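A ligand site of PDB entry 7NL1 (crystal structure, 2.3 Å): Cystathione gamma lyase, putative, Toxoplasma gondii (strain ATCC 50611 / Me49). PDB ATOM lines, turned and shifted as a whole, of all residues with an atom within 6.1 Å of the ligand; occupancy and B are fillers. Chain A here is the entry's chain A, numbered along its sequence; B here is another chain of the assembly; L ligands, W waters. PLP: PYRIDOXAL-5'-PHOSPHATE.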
ATOM      1  N   ALA A 106       3.290  17.250  18.001  1.00  0.00           N
ATOM      2  CA  ALA A 106       2.116  16.864  17.221  1.00  0.00           C
ATOM      3  C   ALA A 106       1.951  15.346  17.160  1.00  0.00           C
ATOM      4  O   ALA A 106       0.822  14.858  17.073  1.00  0.00           O
ATOM      5  CB  ALA A 106       2.209  17.437  15.814  1.00  0.00           C
ATOM      6  N   THR A 107       3.044  14.594  17.192  1.00  0.00           N
ATOM      7  CA  THR A 107       3.033  13.137  17.206  1.00  0.00           C
ATOM      8  C   THR A 107       4.169  12.652  18.092  1.00  0.00           C
ATOM      9  O   THR A 107       5.070  13.418  18.463  1.00  0.00           O
ATOM     10  CB  THR A 107       3.203  12.529  15.806  1.00  0.00           C
ATOM     11  OG1 THR A 107       4.490  12.907  15.296  1.00  0.00           O
ATOM     12  CG2 THR A 107       2.111  12.990  14.851  1.00  0.00           C
ATOM     13  N   GLY A 108       4.135  11.364  18.429  1.00  0.00           N
ATOM     14  CA  GLY A 108       5.285  10.755  19.074  1.00  0.00           C
ATOM     15  C   GLY A 108       6.503  10.725  18.168  1.00  0.00           C
ATOM     16  O   GLY A 108       7.646  10.919  18.625  1.00  0.00           O
ATOM     17  N   MET A 109       6.298  10.473  16.869  1.00  0.00           N
ATOM     18  CA  MET A 109       7.400  10.516  15.915  1.00  0.00           C
ATOM     19  C   MET A 109       8.047  11.891  15.906  1.00  0.00           C
ATOM     20  O   MET A 109       9.267  12.012  15.757  1.00  0.00           O
ATOM     21  CB  MET A 109       6.909  10.150  14.514  1.00  0.00           C
ATOM     22  CG  MET A 109       6.739   8.665  14.268  1.00  0.00           C
ATOM     23  SD  MET A 109       8.139   7.667  14.826  1.00  0.00           S
ATOM     24  CE  MET A 109       9.476   8.366  13.869  1.00  0.00           C
ATOM     25  N   ALA A 110       7.244  12.947  16.049  1.00  0.00           N
ATOM     26  CA  ALA A 110       7.803  14.304  16.102  1.00  0.00           C
ATOM     27  C   ALA A 110       8.730  14.451  17.302  1.00  0.00           C
ATOM     28  O   ALA A 110       9.814  15.045  17.188  1.00  0.00           O
ATOM     29  CB  ALA A 110       6.687  15.340  16.161  1.00  0.00           C
ATOM     30  N   THR A 112      10.383  12.005  18.957  1.00  0.00           N
ATOM     31  CA  THR A 112      11.581  11.200  18.729  1.00  0.00           C
ATOM     32  C   THR A 112      12.524  11.881  17.746  1.00  0.00           C
ATOM     33  O   THR A 112      13.746  11.938  17.965  1.00  0.00           O
ATOM     34  CB  THR A 112      11.185   9.815  18.219  1.00  0.00           C
ATOM     35  OG1 THR A 112      10.419   9.139  19.226  1.00  0.00           O
ATOM     36  CG2 THR A 112      12.417   8.975  17.890  1.00  0.00           C
ATOM     37  N   TYR A 133      10.418   0.629  18.259  1.00  0.00           N
ATOM     38  CA  TYR A 133       9.229   0.822  17.459  1.00  0.00           C
ATOM     39  C   TYR A 133       9.632   0.989  15.999  1.00  0.00           C
ATOM     40  O   TYR A 133      10.637   1.630  15.692  1.00  0.00           O
ATOM     41  CB  TYR A 133       8.454   2.046  17.942  1.00  0.00           C
ATOM     42  CG  TYR A 133       7.348   2.463  17.009  1.00  0.00           C
ATOM     43  CD1 TYR A 133       6.320   1.591  16.701  1.00  0.00           C
ATOM     44  CD2 TYR A 133       7.324   3.739  16.448  1.00  0.00           C
ATOM     45  CE1 TYR A 133       5.294   1.963  15.855  1.00  0.00           C
ATOM     46  CE2 TYR A 133       6.305   4.122  15.596  1.00  0.00           C
ATOM     47  CZ  TYR A 133       5.295   3.231  15.309  1.00  0.00           C
ATOM     48  OH  TYR A 133       4.284   3.612  14.462  1.00  0.00           O
ATOM     49  N   THR A 136      10.586   4.498  14.876  1.00  0.00           N
ATOM     50  CA  THR A 136      11.901   4.939  15.349  1.00  0.00           C
ATOM     51  C   THR A 136      13.013   4.370  14.467  1.00  0.00           C
ATOM     52  O   THR A 136      13.898   5.091  13.993  1.00  0.00           O
ATOM     53  CB  THR A 136      12.100   4.531  16.809  1.00  0.00           C
ATOM     54  OG1 THR A 136      10.950   4.901  17.586  1.00  0.00           O
ATOM     55  CG2 THR A 136      13.329   5.198  17.410  1.00  0.00           C
ATOM     56  N   GLU A 176      13.991   1.156  24.903  1.00  0.00           N
ATOM     57  CA  GLU A 176      12.540   1.071  24.848  1.00  0.00           C
ATOM     58  C   GLU A 176      12.096  -0.107  25.705  1.00  0.00           C
ATOM     59  O   GLU A 176      12.659  -1.199  25.590  1.00  0.00           O
ATOM     60  CB  GLU A 176      12.049   0.892  23.401  1.00  0.00           C
ATOM     61  CG  GLU A 176      10.589   1.220  23.181  1.00  0.00           C
ATOM     62  CD  GLU A 176      10.132   0.936  21.764  1.00  0.00           C
ATOM     63  OE1 GLU A 176       9.402  -0.055  21.560  1.00  0.00           O
ATOM     64  OE2 GLU A 176      10.516   1.708  20.858  1.00  0.00           O
ATOM     65  N   PRO A 178       8.241  -1.527  27.814  1.00  0.00           N
ATOM     66  CA  PRO A 178       8.364  -2.734  26.980  1.00  0.00           C
ATOM     67  C   PRO A 178       8.430  -2.398  25.493  1.00  0.00           C
ATOM     68  O   PRO A 178       7.921  -1.352  25.083  1.00  0.00           O
ATOM     69  CB  PRO A 178       7.090  -3.520  27.308  1.00  0.00           C
ATOM     70  CG  PRO A 178       6.557  -2.911  28.574  1.00  0.00           C
ATOM     71  CD  PRO A 178       6.952  -1.480  28.515  1.00  0.00           C
ATOM     72  N   ASN A 180       7.926  -2.480  21.382  1.00  0.00           N
ATOM     73  CA  ASN A 180       6.865  -2.663  20.401  1.00  0.00           C
ATOM     74  C   ASN A 180       7.371  -3.560  19.283  1.00  0.00           C
ATOM     75  O   ASN A 180       8.324  -3.185  18.585  1.00  0.00           O
ATOM     76  CB  ASN A 180       6.441  -1.315  19.834  1.00  0.00           C
ATOM     77  CG  ASN A 180       5.125  -1.380  19.079  1.00  0.00           C
ATOM     78  OD1 ASN A 180       4.678  -2.450  18.683  1.00  0.00           O
ATOM     79  ND2 ASN A 180       4.514  -0.226  18.868  1.00  0.00           N
ATOM     80  N   ASP A 205      12.098   5.310  25.629  1.00  0.00           N
ATOM     81  CA  ASP A 205      10.722   5.351  25.144  1.00  0.00           C
ATOM     82  C   ASP A 205       9.923   4.357  25.974  1.00  0.00           C
ATOM     83  O   ASP A 205      10.052   3.149  25.787  1.00  0.00           O
ATOM     84  CB  ASP A 205      10.678   5.018  23.662  1.00  0.00           C
ATOM     85  CG  ASP A 205       9.288   5.173  23.053  1.00  0.00           C
ATOM     86  OD1 ASP A 205       8.291   5.211  23.799  1.00  0.00           O
ATOM     87  OD2 ASP A 205       9.210   5.249  21.811  1.00  0.00           O
ATOM     88  N   THR A 207       6.513   4.358  26.100  1.00  0.00           N
ATOM     89  CA  THR A 207       5.134   4.508  25.638  1.00  0.00           C
ATOM     90  C   THR A 207       4.283   3.316  26.051  1.00  0.00           C
ATOM     91  O   THR A 207       3.162   3.486  26.540  1.00  0.00           O
ATOM     92  CB  THR A 207       5.114   4.690  24.116  1.00  0.00           C
ATOM     93  OG1 THR A 207       5.646   5.965  23.769  1.00  0.00           O
ATOM     94  CG2 THR A 207       3.702   4.569  23.590  1.00  0.00           C
ATOM     95  N   PHE A 208       4.809   2.095  25.888  1.00  0.00           N
ATOM     96  CA  PHE A 208       4.061   0.912  26.270  1.00  0.00           C
ATOM     97  C   PHE A 208       3.866   0.823  27.781  1.00  0.00           C
ATOM     98  O   PHE A 208       2.856   0.284  28.238  1.00  0.00           O
ATOM     99  CB  PHE A 208       4.789  -0.345  25.789  1.00  0.00           C
ATOM    100  CG  PHE A 208       4.352  -0.826  24.442  1.00  0.00           C
ATOM    101  CD1 PHE A 208       4.199   0.063  23.394  1.00  0.00           C
ATOM    102  CD2 PHE A 208       4.125  -2.173  24.225  1.00  0.00           C
ATOM    103  CE1 PHE A 208       3.809  -0.388  22.149  1.00  0.00           C
ATOM    104  CE2 PHE A 208       3.730  -2.624  22.988  1.00  0.00           C
ATOM    105  CZ  PHE A 208       3.577  -1.735  21.940  1.00  0.00           C
ATOM    106  N   SER A 227       4.709   8.702  23.347  1.00  0.00           N
ATOM    107  CA  SER A 227       3.715   8.965  22.320  1.00  0.00           C
ATOM    108  C   SER A 227       2.382   9.002  23.053  1.00  0.00           C
ATOM    109  O   SER A 227       1.808   7.965  23.393  1.00  0.00           O
ATOM    110  CB  SER A 227       3.729   7.922  21.219  1.00  0.00           C
ATOM    111  OG  SER A 227       2.448   7.739  20.634  1.00  0.00           O
ATOM    112  N   THR A 228       1.896  10.221  23.334  1.00  0.00           N
ATOM    113  CA  THR A 228       0.635  10.367  24.040  1.00  0.00           C
ATOM    114  C   THR A 228      -0.552   9.863  23.239  1.00  0.00           C
ATOM    115  O   THR A 228      -1.651   9.745  23.788  1.00  0.00           O
ATOM    116  CB  THR A 228       0.419  11.838  24.419  1.00  0.00           C
ATOM    117  OG1 THR A 228       0.132  12.593  23.241  1.00  0.00           O
ATOM    118  CG2 THR A 228       1.669  12.391  25.089  1.00  0.00           C
ATOM    119  N   THR A 229      -0.346   9.546  21.954  1.00  0.00           N
ATOM    120  CA  THR A 229      -1.373   8.913  21.138  1.00  0.00           C
ATOM    121  C   THR A 229      -1.907   7.637  21.764  1.00  0.00           C
ATOM    122  O   THR A 229      -3.091   7.310  21.606  1.00  0.00           O
ATOM    123  CB  THR A 229      -0.787   8.613  19.754  1.00  0.00           C
ATOM    124  OG1 THR A 229      -0.304   9.818  19.158  1.00  0.00           O
ATOM    125  CG2 THR A 229      -1.831   7.994  18.847  1.00  0.00           C
ATOM    126  N   LYS A 230      -1.070   6.907  22.500  1.00  0.00           N
ATOM    127  CA  LYS A 230      -1.435   5.571  22.939  1.00  0.00           C
ATOM    128  C   LYS A 230      -2.224   5.570  24.248  1.00  0.00           C
ATOM    129  O   LYS A 230      -3.455   5.481  24.220  1.00  0.00           O
ATOM    130  CB  LYS A 230      -0.172   4.705  23.070  1.00  0.00           C
ATOM    131  CG  LYS A 230       0.725   4.737  21.818  1.00  0.00           C
ATOM    132  CD  LYS A 230      -0.068   4.628  20.526  1.00  0.00           C
ATOM    133  CE  LYS A 230       0.724   3.927  19.426  1.00  0.00           C
ATOM    134  NZ  LYS A 230       2.144   4.356  19.363  1.00  0.00           N
ATOM    135  N   LEU A 239      -3.583  12.461  18.128  1.00  0.00           N
ATOM    136  CA  LEU A 239      -2.155  12.207  17.999  1.00  0.00           C
ATOM    137  C   LEU A 239      -1.398  13.169  18.905  1.00  0.00           C
ATOM    138  O   LEU A 239      -1.828  14.308  19.127  1.00  0.00           O
ATOM    139  CB  LEU A 239      -1.687  12.389  16.556  1.00  0.00           C
ATOM    140  CG  LEU A 239      -2.364  11.595  15.449  1.00  0.00           C
ATOM    141  CD1 LEU A 239      -2.005  12.212  14.100  1.00  0.00           C
ATOM    142  CD2 LEU A 239      -1.912  10.139  15.505  1.00  0.00           C
ATOM    143  N   GLY A 240      -0.259  12.716  19.421  1.00  0.00           N
ATOM    144  CA  GLY A 240       0.564  13.572  20.236  1.00  0.00           C
ATOM    145  C   GLY A 240       1.830  12.923  20.735  1.00  0.00           C
ATOM    146  O   GLY A 240       1.903  11.698  20.851  1.00  0.00           O
ATOM    147  N   GLY A 241       2.848  13.738  21.030  1.00  0.00           N
ATOM    148  CA  GLY A 241       4.083  13.249  21.587  1.00  0.00           C
ATOM    149  C   GLY A 241       4.528  14.110  22.764  1.00  0.00           C
ATOM    150  O   GLY A 241       3.986  15.191  23.006  1.00  0.00           O
ATOM    151  N   ASN A 360      -3.641   0.964  16.108  1.00  0.00           N
ATOM    152  CA  ASN A 360      -3.268   1.686  17.318  1.00  0.00           C
ATOM    153  C   ASN A 360      -3.082   0.723  18.481  1.00  0.00           C
ATOM    154  O   ASN A 360      -3.125  -0.496  18.342  1.00  0.00           O
ATOM    155  CB  ASN A 360      -4.315   2.756  17.633  1.00  0.00           C
ATOM    156  CG  ASN A 360      -3.754   3.914  18.424  1.00  0.00           C
ATOM    157  OD1 ASN A 360      -2.537   4.087  18.501  1.00  0.00           O
ATOM    158  ND2 ASN A 360      -4.640   4.714  19.024  1.00  0.00           N
ATOM    159  N   LEU A 361      -2.867   1.302  19.662  1.00  0.00           N
ATOM    160  CA  LEU A 361      -2.806   0.542  20.904  1.00  0.00           C
ATOM    161  C   LEU A 361      -3.064   1.488  22.071  1.00  0.00           C
ATOM    162  O   LEU A 361      -2.951   2.711  21.959  1.00  0.00           O
ATOM    163  CB  LEU A 361      -1.465  -0.164  21.089  1.00  0.00           C
ATOM    164  CG  LEU A 361      -0.209   0.699  21.215  1.00  0.00           C
ATOM    165  CD1 LEU A 361       0.295   0.803  22.662  1.00  0.00           C
ATOM    166  CD2 LEU A 361       0.894   0.169  20.309  1.00  0.00           C
ATOM    167  N   TYR B  78      -3.794   5.206   9.680  1.00  0.00           N
ATOM    168  CA  TYR B  78      -3.293   5.855  10.876  1.00  0.00           C
ATOM    169  C   TYR B  78      -3.148   7.340  10.593  1.00  0.00           C
ATOM    170  O   TYR B  78      -2.594   7.728   9.554  1.00  0.00           O
ATOM    171  CB  TYR B  78      -1.955   5.231  11.302  1.00  0.00           C
ATOM    172  CG  TYR B  78      -1.478   5.594  12.682  1.00  0.00           C
ATOM    173  CD1 TYR B  78      -2.097   5.051  13.816  1.00  0.00           C
ATOM    174  CD2 TYR B  78      -0.393   6.432  12.868  1.00  0.00           C
ATOM    175  CE1 TYR B  78      -1.642   5.370  15.084  1.00  0.00           C
ATOM    176  CE2 TYR B  78       0.066   6.742  14.126  1.00  0.00           C
ATOM    177  CZ  TYR B  78      -0.558   6.216  15.235  1.00  0.00           C
ATOM    178  OH  TYR B  78      -0.092   6.537  16.487  1.00  0.00           O
ATOM    179  N   ARG B  80      -1.371   9.803  11.610  1.00  0.00           N
ATOM    180  CA  ARG B  80      -0.078  10.439  11.379  1.00  0.00           C
ATOM    181  C   ARG B  80       0.315  10.360   9.908  1.00  0.00           C
ATOM    182  O   ARG B  80       0.952  11.280   9.392  1.00  0.00           O
ATOM    183  CB  ARG B  80       1.000   9.789  12.257  1.00  0.00           C
ATOM    184  CG  ARG B  80       2.421  10.061  11.789  1.00  0.00           C
ATOM    185  CD  ARG B  80       3.425   9.927  12.931  1.00  0.00           C
ATOM    186  NE  ARG B  80       3.347   8.648  13.630  1.00  0.00           N
ATOM    187  CZ  ARG B  80       3.641   7.468  13.099  1.00  0.00           C
ATOM    188  NH1 ARG B  80       3.656   6.386  13.866  1.00  0.00           N
ATOM    189  NH2 ARG B  80       4.014   7.369  11.824  1.00  0.00           N
ATOM    190  N   GLY B 262       6.487  13.037  11.422  1.00  0.00           N
ATOM    191  CA  GLY B 262       5.352  13.192  12.311  1.00  0.00           C
ATOM    192  C   GLY B 262       4.902  14.620  12.556  1.00  0.00           C
ATOM    193  O   GLY B 262       4.478  14.953  13.667  1.00  0.00           O
HETATM  194  N1  PLP L   1       7.108   4.880  20.026  1.00  0.00           N
HETATM  195  C2  PLP L   1       6.363   3.859  20.383  1.00  0.00           C
HETATM  196  C2A PLP L   1       6.879   2.857  21.421  1.00  0.00           C
HETATM  197  C3  PLP L   1       5.100   3.676  19.832  1.00  0.00           C
HETATM  198  O3  PLP L   1       4.309   2.585  20.212  1.00  0.00           O
HETATM  199  C4  PLP L   1       4.642   4.593  18.899  1.00  0.00           C
HETATM  200  C4A PLP L   1       3.259   4.418  18.267  1.00  0.00           C
HETATM  201  C5  PLP L   1       5.468   5.660  18.550  1.00  0.00           C
HETATM  202  C6  PLP L   1       6.708   5.774  19.148  1.00  0.00           C
HETATM  203  C5A PLP L   1       5.027   6.699  17.525  1.00  0.00           C
HETATM  204  O4P PLP L   1       4.156   7.609  18.136  1.00  0.00           O
HETATM  205  P   PLP L   1       3.063   8.410  17.198  1.00  0.00           P
HETATM  206  O1P PLP L   1       2.202   9.262  18.100  1.00  0.00           O
HETATM  207  O2P PLP L   1       2.197   7.417  16.469  1.00  0.00           O
HETATM  208  O3P PLP L   1       3.800   9.276  16.198  1.00  0.00           O
HETATM  209  O   HOH W   1       9.231   7.225  17.854  1.00  0.00           O
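Residues that only touch the ligand: Thr 107 (3.3 Å), Tyr 133 (3.4 Å), Glu 176 (3.8 Å), Thr 207 (3.7 Å), Phe 208 (3.6 Å) and Gly 240 (3.7 Å). Hydrophobic or aromatic side chains within 4 Å of the ligand: Met 109, Tyr 133, Phe 208 and Tyr 78 of chain B. 15 residues have an atom within 4 Å of the ligand: Thr 107, Gly 108, Met 109, Tyr 133, Glu 176, Asn 180, Asp 205, Thr 207, Phe 208, Ser 227, Thr 229, Lys 230, Gly 240, Tyr 78 of chain B and Arg 80 of chain B.
The guanidinium group (NH1) of Arg 80 of chain B lies within hydrogen-bond range of the side-chain hydroxyl (OH) of Tyr 133 (2.9 Å). OD1 of Asp 205 is in hydrogen-bond range of OG1 of Thr 207 (2.8 Å). The side-chain hydroxyl of Thr 107 lies close to the backbone NH of Met 109, 3.4 Å away. O of Gly 240 lies within hydrogen-bond range of N of Gly 108 (3.3 Å). N of Ser 227 lies within hydrogen-bond range of OG1 of Thr 207 (2.9 Å). The backbone carbonyl oxygen (O) of Thr 107 lies close to the backbone NH (N) of Gly 241 (3.4 Å). The side-chain hydroxyl (OG1) of Thr 107 is in hydrogen-bond range of the backbone carbonyl oxygen (O) of Gly 262 of chain B (2.6 Å). OE2 of Glu 176 lies within hydrogen-bond range of N of Tyr 133, at 2.8 Å.
NZ of Lys 230 is covalently linked to C4A of the ligand, 1.6 Å away. The side-chain hydroxyl (OH) of Tyr 78 of chain B sits at hydrogen-bond distance from an oxygen (O2P) of the ligand. An oxygen (O3P) of the ligand lies within salt-bridge range of the guanidinium group (NE) of Arg 80 of chain B, at 2.7 Å. The side-chain hydroxyl (OG1) of Thr 229 sits at hydrogen-bond distance from an oxygen (O1P) of the ligand (2.8 Å). OD2 of Asp 205 sits at hydrogen-bond distance from N1 of the ligand, 2.8 Å away. The backbone NH (N) of Met 109 lies within hydrogen-bond range of an oxygen (O3P) of the ligand, 2.9 Å away. An oxygen (O1P) of the ligand lies within hydrogen-bond range of the backbone NH (N) of Gly 108 (2.9 Å). The side-chain hydroxyl (OG) of Ser 227 sits at hydrogen-bond distance from an oxygen (O1P) of the ligand (3.0 Å). ND2 of Asn 180 sits at hydrogen-bond distance from O3 of the ligand (3.1 Å).
Water W1 lies within hydrogen-bond range of the side-chain hydroxyl (OG1) of Thr 112 (2.6 Å), the side-chain hydroxyl (OG1) of Thr 136 (2.9 Å) and the side-chain sulfur (SD) of Met 109 (3.2 Å).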
